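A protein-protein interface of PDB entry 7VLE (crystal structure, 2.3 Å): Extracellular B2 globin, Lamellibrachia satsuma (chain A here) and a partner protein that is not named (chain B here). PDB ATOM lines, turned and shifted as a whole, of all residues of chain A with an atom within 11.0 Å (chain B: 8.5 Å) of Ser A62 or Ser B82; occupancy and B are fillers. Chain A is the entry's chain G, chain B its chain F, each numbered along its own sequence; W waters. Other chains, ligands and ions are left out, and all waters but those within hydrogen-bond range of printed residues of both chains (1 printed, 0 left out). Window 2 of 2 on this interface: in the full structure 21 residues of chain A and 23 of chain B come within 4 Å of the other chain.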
ATOM      1  N   THR A  26      -8.967 -11.546   4.057  1.00  0.00           N
ATOM      2  CA  THR A  26      -9.046 -11.567   5.511  1.00  0.00           C
ATOM      3  C   THR A  26      -7.928 -12.376   6.148  1.00  0.00           C
ATOM      4  O   THR A  26      -7.870 -12.450   7.380  1.00  0.00           O
ATOM      5  CB  THR A  26     -10.396 -12.131   5.962  1.00  0.00           C
ATOM      6  OG1 THR A  26     -10.469 -13.525   5.633  1.00  0.00           O
ATOM      7  CG2 THR A  26     -11.530 -11.397   5.275  1.00  0.00           C
ATOM      8  N   LEU A  30      -7.627 -11.737   9.921  1.00  0.00           N
ATOM      9  CA  LEU A  30      -8.100 -12.760  10.845  1.00  0.00           C
ATOM     10  C   LEU A  30      -7.037 -13.111  11.874  1.00  0.00           C
ATOM     11  O   LEU A  30      -7.347 -13.316  13.054  1.00  0.00           O
ATOM     12  CB  LEU A  30      -8.515 -13.999  10.055  1.00  0.00           C
ATOM     13  CG  LEU A  30      -9.508 -14.965  10.690  1.00  0.00           C
ATOM     14  CD1 LEU A  30     -10.673 -14.192  11.276  1.00  0.00           C
ATOM     15  CD2 LEU A  30      -9.995 -15.955   9.644  1.00  0.00           C
ATOM     16  N   GLN A  34      -7.609 -12.832  15.933  1.00  0.00           N
ATOM     17  CA  GLN A  34      -7.485 -14.071  16.694  1.00  0.00           C
ATOM     18  C   GLN A  34      -6.384 -13.966  17.740  1.00  0.00           C
ATOM     19  O   GLN A  34      -6.574 -14.367  18.894  1.00  0.00           O
ATOM     20  CB  GLN A  34      -7.216 -15.244  15.749  1.00  0.00           C
ATOM     21  CG  GLN A  34      -8.426 -15.689  14.944  1.00  0.00           C
ATOM     22  CD  GLN A  34      -8.099 -16.802  13.964  1.00  0.00           C
ATOM     23  OE1 GLN A  34      -7.015 -16.832  13.377  1.00  0.00           O
ATOM     24  NE2 GLN A  34      -9.034 -17.726  13.784  1.00  0.00           N
ATOM     25  N   PHE A  51     -18.818 -14.169  24.824  1.00  0.00           N
ATOM     26  CA  PHE A  51     -18.900 -14.463  23.399  1.00  0.00           C
ATOM     27  C   PHE A  51     -19.457 -15.859  23.151  1.00  0.00           C
ATOM     28  O   PHE A  51     -18.899 -16.621  22.356  1.00  0.00           O
ATOM     29  CB  PHE A  51     -17.519 -14.323  22.754  1.00  0.00           C
ATOM     30  CG  PHE A  51     -16.839 -13.016  23.052  1.00  0.00           C
ATOM     31  CD1 PHE A  51     -17.109 -11.891  22.291  1.00  0.00           C
ATOM     32  CD2 PHE A  51     -15.927 -12.912  24.090  1.00  0.00           C
ATOM     33  CE1 PHE A  51     -16.486 -10.688  22.560  1.00  0.00           C
ATOM     34  CE2 PHE A  51     -15.299 -11.711  24.364  1.00  0.00           C
ATOM     35  CZ  PHE A  51     -15.580 -10.598  23.598  1.00  0.00           C
ATOM     36  N   ASP A  52     -20.554 -16.205  23.830  1.00  0.00           N
ATOM     37  CA  ASP A  52     -21.173 -17.509  23.613  1.00  0.00           C
ATOM     38  C   ASP A  52     -21.881 -17.565  22.266  1.00  0.00           C
ATOM     39  O   ASP A  52     -21.794 -18.573  21.552  1.00  0.00           O
ATOM     40  CB  ASP A  52     -22.159 -17.819  24.740  1.00  0.00           C
ATOM     41  CG  ASP A  52     -21.477 -18.014  26.077  1.00  0.00           C
ATOM     42  OD1 ASP A  52     -20.236 -18.158  26.101  1.00  0.00           O
ATOM     43  OD2 ASP A  52     -22.184 -18.021  27.107  1.00  0.00           O
ATOM     44  N   ARG A  53     -22.588 -16.490  21.906  1.00  0.00           N
ATOM     45  CA  ARG A  53     -23.351 -16.467  20.662  1.00  0.00           C
ATOM     46  C   ARG A  53     -22.444 -16.625  19.450  1.00  0.00           C
ATOM     47  O   ARG A  53     -22.814 -17.277  18.466  1.00  0.00           O
ATOM     48  CB  ARG A  53     -24.145 -15.166  20.565  1.00  0.00           C
ATOM     49  CG  ARG A  53     -25.184 -15.154  19.460  1.00  0.00           C
ATOM     50  CD  ARG A  53     -25.726 -13.754  19.220  1.00  0.00           C
ATOM     51  NE  ARG A  53     -24.796 -12.935  18.448  1.00  0.00           N
ATOM     52  CZ  ARG A  53     -24.780 -12.881  17.120  1.00  0.00           C
ATOM     53  NH1 ARG A  53     -23.900 -12.109  16.495  1.00  0.00           N
ATOM     54  NH2 ARG A  53     -25.643 -13.599  16.416  1.00  0.00           N
ATOM     55  N   VAL A  54     -21.255 -16.025  19.498  1.00  0.00           N
ATOM     56  CA  VAL A  54     -20.291 -16.117  18.409  1.00  0.00           C
ATOM     57  C   VAL A  54     -19.218 -17.165  18.686  1.00  0.00           C
ATOM     58  O   VAL A  54     -18.182 -17.174  18.017  1.00  0.00           O
ATOM     59  CB  VAL A  54     -19.654 -14.750  18.117  1.00  0.00           C
ATOM     60  CG1 VAL A  54     -20.716 -13.752  17.678  1.00  0.00           C
ATOM     61  CG2 VAL A  54     -18.909 -14.242  19.342  1.00  0.00           C
ATOM     62  N   HIS A  55     -19.435 -18.038  19.672  1.00  0.00           N
ATOM     63  CA  HIS A  55     -18.575 -19.193  19.935  1.00  0.00           C
ATOM     64  C   HIS A  55     -17.157 -18.763  20.326  1.00  0.00           C
ATOM     65  O   HIS A  55     -16.174 -19.108  19.671  1.00  0.00           O
ATOM     66  CB  HIS A  55     -18.529 -20.137  18.727  1.00  0.00           C
ATOM     67  CG  HIS A  55     -19.863 -20.671  18.307  1.00  0.00           C
ATOM     68  ND1 HIS A  55     -20.004 -21.890  17.679  1.00  0.00           N
ATOM     69  CD2 HIS A  55     -21.111 -20.152  18.407  1.00  0.00           C
ATOM     70  CE1 HIS A  55     -21.282 -22.103  17.417  1.00  0.00           C
ATOM     71  NE2 HIS A  55     -21.974 -21.064  17.849  1.00  0.00           N
ATOM     72  N   GLY A  56     -17.065 -18.013  21.425  1.00  0.00           N
ATOM     73  CA  GLY A  56     -15.764 -17.576  21.906  1.00  0.00           C
ATOM     74  C   GLY A  56     -14.871 -18.700  22.393  1.00  0.00           C
ATOM     75  O   GLY A  56     -13.660 -18.499  22.537  1.00  0.00           O
ATOM     76  N   THR A  57     -15.443 -19.878  22.656  1.00  0.00           N
ATOM     77  CA  THR A  57     -14.657 -21.028  23.088  1.00  0.00           C
ATOM     78  C   THR A  57     -13.953 -21.697  21.919  1.00  0.00           C
ATOM     79  O   THR A  57     -12.921 -22.352  22.107  1.00  0.00           O
ATOM     80  CB  THR A  57     -15.553 -22.042  23.798  1.00  0.00           C
ATOM     81  OG1 THR A  57     -16.547 -22.522  22.882  1.00  0.00           O
ATOM     82  CG2 THR A  57     -16.241 -21.397  24.988  1.00  0.00           C
ATOM     83  N   GLU A  58     -14.505 -21.551  20.723  1.00  0.00           N
ATOM     84  CA  GLU A  58     -13.910 -22.061  19.496  1.00  0.00           C
ATOM     85  C   GLU A  58     -13.360 -20.863  18.730  1.00  0.00           C
ATOM     86  O   GLU A  58     -14.107 -20.141  18.063  1.00  0.00           O
ATOM     87  CB  GLU A  58     -14.934 -22.848  18.684  1.00  0.00           C
ATOM     88  CG  GLU A  58     -14.357 -23.582  17.489  1.00  0.00           C
ATOM     89  CD  GLU A  58     -13.139 -24.423  17.823  1.00  0.00           C
ATOM     90  OE1 GLU A  58     -12.935 -24.776  19.006  1.00  0.00           O
ATOM     91  OE2 GLU A  58     -12.377 -24.742  16.888  1.00  0.00           O
ATOM     92  N   ILE A  59     -12.046 -20.652  18.841  1.00  0.00           N
ATOM     93  CA  ILE A  59     -11.430 -19.468  18.254  1.00  0.00           C
ATOM     94  C   ILE A  59     -11.412 -19.553  16.734  1.00  0.00           C
ATOM     95  O   ILE A  59     -11.467 -18.526  16.047  1.00  0.00           O
ATOM     96  CB  ILE A  59     -10.014 -19.276  18.825  1.00  0.00           C
ATOM     97  CG1 ILE A  59     -10.064 -19.239  20.352  1.00  0.00           C
ATOM     98  CG2 ILE A  59      -9.381 -18.001  18.281  1.00  0.00           C
ATOM     99  CD1 ILE A  59      -8.743 -19.547  21.011  1.00  0.00           C
ATOM    100  N   ASP A  60     -11.342 -20.761  16.177  1.00  0.00           N
ATOM    101  CA  ASP A  60     -11.225 -20.925  14.736  1.00  0.00           C
ATOM    102  C   ASP A  60     -12.522 -21.409  14.093  1.00  0.00           C
ATOM    103  O   ASP A  60     -12.491 -21.970  12.994  1.00  0.00           O
ATOM    104  CB  ASP A  60     -10.066 -21.866  14.405  1.00  0.00           C
ATOM    105  CG  ASP A  60      -9.375 -21.499  13.107  1.00  0.00           C
ATOM    106  OD1 ASP A  60      -9.501 -22.259  12.124  1.00  0.00           O
ATOM    107  OD2 ASP A  60      -8.723 -20.434  13.063  1.00  0.00           O
ATOM    108  N   SER A  61     -13.658 -21.199  14.753  1.00  0.00           N
ATOM    109  CA  SER A  61     -14.944 -21.479  14.134  1.00  0.00           C
ATOM    110  C   SER A  61     -15.359 -20.319  13.233  1.00  0.00           C
ATOM    111  O   SER A  61     -14.923 -19.178  13.406  1.00  0.00           O
ATOM    112  CB  SER A  61     -16.025 -21.721  15.188  1.00  0.00           C
ATOM    113  OG  SER A  61     -16.459 -20.505  15.774  1.00  0.00           O
ATOM    114  N   SER A  62     -16.221 -20.630  12.261  1.00  0.00           N
ATOM    115  CA  SER A  62     -16.674 -19.612  11.316  1.00  0.00           C
ATOM    116  C   SER A  62     -17.380 -18.469  12.033  1.00  0.00           C
ATOM    117  O   SER A  62     -17.168 -17.295  11.705  1.00  0.00           O
ATOM    118  CB  SER A  62     -17.604 -20.238  10.277  1.00  0.00           C
ATOM    119  OG  SER A  62     -16.954 -21.270   9.559  1.00  0.00           O
ATOM    120  N   GLU A  63     -18.222 -18.798  13.015  1.00  0.00           N
ATOM    121  CA  GLU A  63     -18.968 -17.779  13.744  1.00  0.00           C
ATOM    122  C   GLU A  63     -18.037 -16.827  14.483  1.00  0.00           C
ATOM    123  O   GLU A  63     -18.303 -15.622  14.558  1.00  0.00           O
ATOM    124  CB  GLU A  63     -19.935 -18.442  14.725  1.00  0.00           C
ATOM    125  CG  GLU A  63     -20.993 -19.325  14.078  1.00  0.00           C
ATOM    126  CD  GLU A  63     -20.496 -20.725  13.761  1.00  0.00           C
ATOM    127  OE1 GLU A  63     -19.300 -21.006  13.985  1.00  0.00           O
ATOM    128  OE2 GLU A  63     -21.308 -21.547  13.287  1.00  0.00           O
ATOM    129  N   PHE A  64     -16.947 -17.350  15.047  1.00  0.00           N
ATOM    130  CA  PHE A  64     -16.006 -16.486  15.750  1.00  0.00           C
ATOM    131  C   PHE A  64     -15.036 -15.807  14.795  1.00  0.00           C
ATOM    132  O   PHE A  64     -14.596 -14.683  15.063  1.00  0.00           O
ATOM    133  CB  PHE A  64     -15.233 -17.275  16.806  1.00  0.00           C
ATOM    134  CG  PHE A  64     -14.391 -16.411  17.697  1.00  0.00           C
ATOM    135  CD1 PHE A  64     -14.983 -15.587  18.638  1.00  0.00           C
ATOM    136  CD2 PHE A  64     -13.012 -16.409  17.585  1.00  0.00           C
ATOM    137  CE1 PHE A  64     -14.215 -14.782  19.457  1.00  0.00           C
ATOM    138  CE2 PHE A  64     -12.236 -15.608  18.403  1.00  0.00           C
ATOM    139  CZ  PHE A  64     -12.839 -14.794  19.339  1.00  0.00           C
ATOM    140  N   LYS A  65     -14.674 -16.481  13.698  1.00  0.00           N
ATOM    141  CA  LYS A  65     -13.961 -15.815  12.612  1.00  0.00           C
ATOM    142  C   LYS A  65     -14.725 -14.589  12.141  1.00  0.00           C
ATOM    143  O   LYS A  65     -14.137 -13.526  11.906  1.00  0.00           O
ATOM    144  CB  LYS A  65     -13.765 -16.775  11.438  1.00  0.00           C
ATOM    145  CG  LYS A  65     -12.670 -17.806  11.607  1.00  0.00           C
ATOM    146  CD  LYS A  65     -12.593 -18.695  10.373  1.00  0.00           C
ATOM    147  CE  LYS A  65     -11.452 -19.690  10.473  1.00  0.00           C
ATOM    148  NZ  LYS A  65     -11.448 -20.645   9.330  1.00  0.00           N
ATOM    149  N   ALA A  66     -16.043 -14.729  11.984  1.00  0.00           N
ATOM    150  CA  ALA A  66     -16.878 -13.616  11.551  1.00  0.00           C
ATOM    151  C   ALA A  66     -16.836 -12.471  12.549  1.00  0.00           C
ATOM    152  O   ALA A  66     -16.773 -11.301  12.159  1.00  0.00           O
ATOM    153  CB  ALA A  66     -18.314 -14.093  11.345  1.00  0.00           C
ATOM    154  N   HIS A  67     -16.882 -12.786  13.842  1.00  0.00           N
ATOM    155  CA  HIS A  67     -16.837 -11.738  14.857  1.00  0.00           C
ATOM    156  C   HIS A  67     -15.517 -10.986  14.804  1.00  0.00           C
ATOM    157  O   HIS A  67     -15.488  -9.756  14.820  1.00  0.00           O
ATOM    158  CB  HIS A  67     -17.061 -12.328  16.249  1.00  0.00           C
ATOM    159  CG  HIS A  67     -16.835 -11.342  17.348  1.00  0.00           C
ATOM    160  ND1 HIS A  67     -17.752 -10.372  17.675  1.00  0.00           N
ATOM    161  CD2 HIS A  67     -15.779 -11.148  18.168  1.00  0.00           C
ATOM    162  CE1 HIS A  67     -17.281  -9.635  18.663  1.00  0.00           C
ATOM    163  NE2 HIS A  67     -16.085 -10.086  18.983  1.00  0.00           N
ATOM    164  N   CYS A  68     -14.415 -11.725  14.742  1.00  0.00           N
ATOM    165  CA  CYS A  68     -13.084 -11.148  14.585  1.00  0.00           C
ATOM    166  C   CYS A  68     -13.021 -10.187  13.402  1.00  0.00           C
ATOM    167  O   CYS A  68     -12.477  -9.081  13.508  1.00  0.00           O
ATOM    168  CB  CYS A  68     -12.056 -12.267  14.407  1.00  0.00           C
ATOM    169  SG  CYS A  68     -11.573 -13.086  15.935  1.00  0.00           S
ATOM    170  N   ILE A  69     -13.558 -10.607  12.255  1.00  0.00           N
ATOM    171  CA  ILE A  69     -13.557  -9.754  11.072  1.00  0.00           C
ATOM    172  C   ILE A  69     -14.443  -8.535  11.292  1.00  0.00           C
ATOM    173  O   ILE A  69     -14.135  -7.430  10.829  1.00  0.00           O
ATOM    174  CB  ILE A  69     -13.988 -10.572   9.839  1.00  0.00           C
ATOM    175  CG1 ILE A  69     -12.865 -11.528   9.428  1.00  0.00           C
ATOM    176  CG2 ILE A  69     -14.387  -9.665   8.683  1.00  0.00           C
ATOM    177  CD1 ILE A  69     -13.273 -12.536   8.391  1.00  0.00           C
ATOM    178  N   ARG A  70     -15.550  -8.710  12.020  1.00  0.00           N
ATOM    179  CA  ARG A  70     -16.393  -7.572  12.368  1.00  0.00           C
ATOM    180  C   ARG A  70     -15.677  -6.619  13.319  1.00  0.00           C
ATOM    181  O   ARG A  70     -15.847  -5.399  13.224  1.00  0.00           O
ATOM    182  CB  ARG A  70     -17.706  -8.057  12.986  1.00  0.00           C
ATOM    183  CG  ARG A  70     -18.710  -8.606  11.987  1.00  0.00           C
ATOM    184  CD  ARG A  70     -20.090  -8.744  12.612  1.00  0.00           C
ATOM    185  NE  ARG A  70     -20.120  -9.727  13.693  1.00  0.00           N
ATOM    186  CZ  ARG A  70     -20.357 -11.022  13.516  1.00  0.00           C
ATOM    187  NH1 ARG A  70     -20.581 -11.498  12.298  1.00  0.00           N
ATOM    188  NH2 ARG A  70     -20.368 -11.846  14.555  1.00  0.00           N
ATOM    189  N   VAL A  71     -14.869  -7.158  14.237  1.00  0.00           N
ATOM    190  CA  VAL A  71     -14.187  -6.322  15.223  1.00  0.00           C
ATOM    191  C   VAL A  71     -13.154  -5.430  14.549  1.00  0.00           C
ATOM    192  O   VAL A  71     -13.147  -4.208  14.742  1.00  0.00           O
ATOM    193  CB  VAL A  71     -13.532  -7.189  16.312  1.00  0.00           C
ATOM    194  CG1 VAL A  71     -12.649  -6.327  17.204  1.00  0.00           C
ATOM    195  CG2 VAL A  71     -14.580  -7.889  17.138  1.00  0.00           C
ATOM    196  N   LEU B  77     -14.155 -11.557   1.978  1.00  0.00           N
ATOM    197  CA  LEU B  77     -14.505 -12.933   2.296  1.00  0.00           C
ATOM    198  C   LEU B  77     -15.063 -13.690   1.099  1.00  0.00           C
ATOM    199  O   LEU B  77     -15.520 -14.827   1.258  1.00  0.00           O
ATOM    200  CB  LEU B  77     -15.511 -12.963   3.446  1.00  0.00           C
ATOM    201  CG  LEU B  77     -14.922 -12.751   4.838  1.00  0.00           C
ATOM    202  CD1 LEU B  77     -16.022 -12.509   5.858  1.00  0.00           C
ATOM    203  CD2 LEU B  77     -14.086 -13.960   5.219  1.00  0.00           C
ATOM    204  N   LEU B  78     -15.034 -13.087  -0.093  1.00  0.00           N
ATOM    205  CA  LEU B  78     -15.557 -13.741  -1.288  1.00  0.00           C
ATOM    206  C   LEU B  78     -14.850 -15.055  -1.591  1.00  0.00           C
ATOM    207  O   LEU B  78     -15.433 -15.920  -2.253  1.00  0.00           O
ATOM    208  CB  LEU B  78     -15.440 -12.804  -2.489  1.00  0.00           C
ATOM    209  CG  LEU B  78     -16.495 -11.704  -2.580  1.00  0.00           C
ATOM    210  CD1 LEU B  78     -16.117 -10.688  -3.645  1.00  0.00           C
ATOM    211  CD2 LEU B  78     -17.854 -12.316  -2.876  1.00  0.00           C
ATOM    212  N   ASP B  79     -13.616 -15.220  -1.129  1.00  0.00           N
ATOM    213  CA  ASP B  79     -12.862 -16.449  -1.319  1.00  0.00           C
ATOM    214  C   ASP B  79     -13.002 -17.409  -0.144  1.00  0.00           C
ATOM    215  O   ASP B  79     -12.343 -18.454  -0.130  1.00  0.00           O
ATOM    216  CB  ASP B  79     -11.387 -16.122  -1.552  1.00  0.00           C
ATOM    217  CG  ASP B  79     -10.734 -15.498  -0.336  1.00  0.00           C
ATOM    218  OD1 ASP B  79      -9.677 -16.002   0.098  1.00  0.00           O
ATOM    219  OD2 ASP B  79     -11.286 -14.516   0.202  1.00  0.00           O
ATOM    220  N   ASP B  80     -13.845 -17.079   0.841  1.00  0.00           N
ATOM    221  CA  ASP B  80     -14.035 -17.900   2.041  1.00  0.00           C
ATOM    222  C   ASP B  80     -15.535 -18.153   2.208  1.00  0.00           C
ATOM    223  O   ASP B  80     -16.202 -17.484   3.002  1.00  0.00           O
ATOM    224  CB  ASP B  80     -13.430 -17.225   3.260  1.00  0.00           C
ATOM    225  CG  ASP B  80     -13.102 -18.206   4.359  1.00  0.00           C
ATOM    226  OD1 ASP B  80     -13.683 -19.311   4.359  1.00  0.00           O
ATOM    227  OD2 ASP B  80     -12.262 -17.875   5.220  1.00  0.00           O
ATOM    228  N   GLU B  81     -16.040 -19.148   1.473  1.00  0.00           N
ATOM    229  CA  GLU B  81     -17.476 -19.404   1.378  1.00  0.00           C
ATOM    230  C   GLU B  81     -18.126 -19.569   2.749  1.00  0.00           C
ATOM    231  O   GLU B  81     -19.179 -18.983   3.026  1.00  0.00           O
ATOM    232  CB  GLU B  81     -17.713 -20.653   0.529  1.00  0.00           C
ATOM    233  CG  GLU B  81     -19.168 -20.935   0.223  1.00  0.00           C
ATOM    234  CD  GLU B  81     -19.756 -19.924  -0.734  1.00  0.00           C
ATOM    235  OE1 GLU B  81     -20.971 -19.652  -0.645  1.00  0.00           O
ATOM    236  OE2 GLU B  81     -18.996 -19.395  -1.574  1.00  0.00           O
ATOM    237  N   SER B  82     -17.516 -20.383   3.612  1.00  0.00           N
ATOM    238  CA  SER B  82     -18.085 -20.645   4.932  1.00  0.00           C
ATOM    239  C   SER B  82     -18.221 -19.362   5.742  1.00  0.00           C
ATOM    240  O   SER B  82     -19.292 -19.063   6.284  1.00  0.00           O
ATOM    241  CB  SER B  82     -17.216 -21.661   5.676  1.00  0.00           C
ATOM    242  OG  SER B  82     -17.555 -21.719   7.050  1.00  0.00           O
ATOM    243  N   VAL B  83     -17.136 -18.590   5.836  1.00  0.00           N
ATOM    244  CA  VAL B  83     -17.155 -17.359   6.620  1.00  0.00           C
ATOM    245  C   VAL B  83     -17.950 -16.273   5.907  1.00  0.00           C
ATOM    246  O   VAL B  83     -18.525 -15.389   6.555  1.00  0.00           O
ATOM    247  CB  VAL B  83     -15.714 -16.903   6.916  1.00  0.00           C
ATOM    248  CG1 VAL B  83     -15.705 -15.798   7.962  1.00  0.00           C
ATOM    249  CG2 VAL B  83     -14.865 -18.083   7.364  1.00  0.00           C
ATOM    250  N   LEU B  84     -17.989 -16.311   4.574  1.00  0.00           N
ATOM    251  CA  LEU B  84     -18.778 -15.340   3.821  1.00  0.00           C
ATOM    252  C   LEU B  84     -20.256 -15.447   4.173  1.00  0.00           C
ATOM    253  O   LEU B  84     -20.903 -14.449   4.509  1.00  0.00           O
ATOM    254  CB  LEU B  84     -18.572 -15.547   2.320  1.00  0.00           C
ATOM    255  CG  LEU B  84     -19.558 -14.829   1.395  1.00  0.00           C
ATOM    256  CD1 LEU B  84     -19.368 -13.322   1.468  1.00  0.00           C
ATOM    257  CD2 LEU B  84     -19.428 -15.327  -0.040  1.00  0.00           C
ATOM    258  N   ASN B  85     -20.804 -16.663   4.103  1.00  0.00           N
ATOM    259  CA  ASN B  85     -22.220 -16.868   4.388  1.00  0.00           C
ATOM    260  C   ASN B  85     -22.550 -16.589   5.848  1.00  0.00           C
ATOM    261  O   ASN B  85     -23.672 -16.175   6.159  1.00  0.00           O
ATOM    262  CB  ASN B  85     -22.624 -18.292   4.009  1.00  0.00           C
ATOM    263  CG  ASN B  85     -22.599 -18.524   2.511  1.00  0.00           C
ATOM    264  OD1 ASN B  85     -22.838 -17.605   1.728  1.00  0.00           O
ATOM    265  ND2 ASN B  85     -22.310 -19.755   2.105  1.00  0.00           N
ATOM    266  N   THR B  86     -21.595 -16.819   6.754  1.00  0.00           N
ATOM    267  CA  THR B  86     -21.793 -16.449   8.152  1.00  0.00           C
ATOM    268  C   THR B  86     -21.975 -14.945   8.292  1.00  0.00           C
ATOM    269  O   THR B  86     -22.863 -14.479   9.017  1.00  0.00           O
ATOM    270  CB  THR B  86     -20.604 -16.917   8.992  1.00  0.00           C
ATOM    271  OG1 THR B  86     -20.419 -18.328   8.826  1.00  0.00           O
ATOM    272  CG2 THR B  86     -20.833 -16.607  10.465  1.00  0.00           C
ATOM    273  N   GLN B  87     -21.137 -14.168   7.602  1.00  0.00           N
ATOM    274  CA  GLN B  87     -21.268 -12.716   7.626  1.00  0.00           C
ATOM    275  C   GLN B  87     -22.491 -12.258   6.842  1.00  0.00           C
ATOM    276  O   GLN B  87     -23.157 -11.292   7.231  1.00  0.00           O
ATOM    277  CB  GLN B  87     -19.997 -12.074   7.070  1.00  0.00           C
ATOM    278  CG  GLN B  87     -20.033 -10.561   7.029  1.00  0.00           C
ATOM    279  CD  GLN B  87     -20.207  -9.950   8.404  1.00  0.00           C
ATOM    280  OE1 GLN B  87     -19.696 -10.470   9.396  1.00  0.00           O
ATOM    281  NE2 GLN B  87     -20.938  -8.844   8.470  1.00  0.00           N
ATOM    282  N   LEU B  88     -22.794 -12.934   5.729  1.00  0.00           N
ATOM    283  CA  LEU B  88     -24.016 -12.635   4.987  1.00  0.00           C
ATOM    284  C   LEU B  88     -25.252 -12.834   5.850  1.00  0.00           C
ATOM    285  O   LEU B  88     -26.246 -12.115   5.691  1.00  0.00           O
ATOM    286  CB  LEU B  88     -24.106 -13.513   3.738  1.00  0.00           C
ATOM    287  CG  LEU B  88     -23.224 -13.155   2.541  1.00  0.00           C
ATOM    288  CD1 LEU B  88     -23.485 -14.108   1.384  1.00  0.00           C
ATOM    289  CD2 LEU B  88     -23.471 -11.718   2.119  1.00  0.00           C
ATOM    290  N   ALA B  89     -25.208 -13.807   6.764  1.00  0.00           N
ATOM    291  CA  ALA B  89     -26.324 -14.038   7.673  1.00  0.00           C
ATOM    292  C   ALA B  89     -26.388 -12.977   8.762  1.00  0.00           C
ATOM    293  O   ALA B  89     -27.482 -12.608   9.203  1.00  0.00           O
ATOM    294  CB  ALA B  89     -26.208 -15.429   8.295  1.00  0.00           C
HETATM  295  O   HOH W   1     -10.339 -14.244   3.325  1.00  0.00           O
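OG of Ser A62 is in hydrogen-bond range of OG of Ser B82, 2.6 Å away.
OE1 of Gln B87 lies within hydrogen-bond range of NH1 of Arg A70.
OG1 of Thr B86 lies within hydrogen-bond range of O of Ser B82, at 2.9 Å.
NZ of Lys A65 lies within salt-bridge range of OD1 of Asp A60.
The side-chain hydroxyl (OG) of Ser A61 is in hydrogen-bond range of the side-chain carboxylate (OE1) of Glu A63.
CG2 of Thr A26 touches CD2 of Leu B77, at 3.6 Å.
CB of Ser A62 touches OG1 of Thr B86, 3.7 Å away.
CA of Glu A63 touches CG2 of Thr B86, at 3.95 Å.
Val B83 touches Lys A65 (CG2 to CD, 3.8 Å).
Thr B86 touches Ala A66 (CG2 to CB, 3.7 Å).
Leu B77 touches Ile A69 (CD2 to CD1, 3.6 Å).
Ser B82 touches just one residue of chain A: Ser A62 (2.6 Å).
No residue of chain B comes within 4 Å of Ser A61.
No residue of chain A comes within 4 Å of Asp B80.
Of chain A, only Lys A65 (3.8 Å) comes within 4 Å of Val B83.
Of chain A, only Ser A62, Glu A63 and Ala A66 come within 4 Å of Thr B86.
Of the printed residues of chain B, Ile A69 touches Leu B77 (3.6 Å).
Printed residues of chain B within 4 Å of Arg A70: Gln B87.
Of the printed residues of chain A, Leu B77 touches Thr A26 and Ile A69.
Printed residues of chain B within 4 Å of Ala A66: Thr B86 (3.7 Å).
Printed residues of chain A within 4 Å of Gln B87: Arg A70 (3.2 Å).
The nearest residue of chain B that does not touch Ser A62 is Val B83 (4.3 Å).
The nearest printed residue of chain B that does not touch Ala A66 is Gln B87 (4.1 Å).
Printed residues of chain A that touch a printed residue of chain B: Thr A26, Ser A62, Glu A63, Lys A65, Ala A66, Ile A69 and Arg A70.
Hydrophobic or aromatic side chains of chain A that line the printed part of chain B: Ala A66 and Ile A69.
Of the 13 printed residues of chain B, 5 touch a printed residue of chain A.
Printed residues of chain B that touch a printed residue of chain A: Leu B77, Ser B82, Val B83, Thr B86 and Gln B87.
Among the printed residues, no Asp or Glu carboxylate lies within 4 Å of a Lys or Arg side-chain nitrogen of the other chain.
Water W1 lies within hydrogen-bond range of OG1 of Thr A26 (2.4 Å) and OD2 of Asp B79 (3.3 Å).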
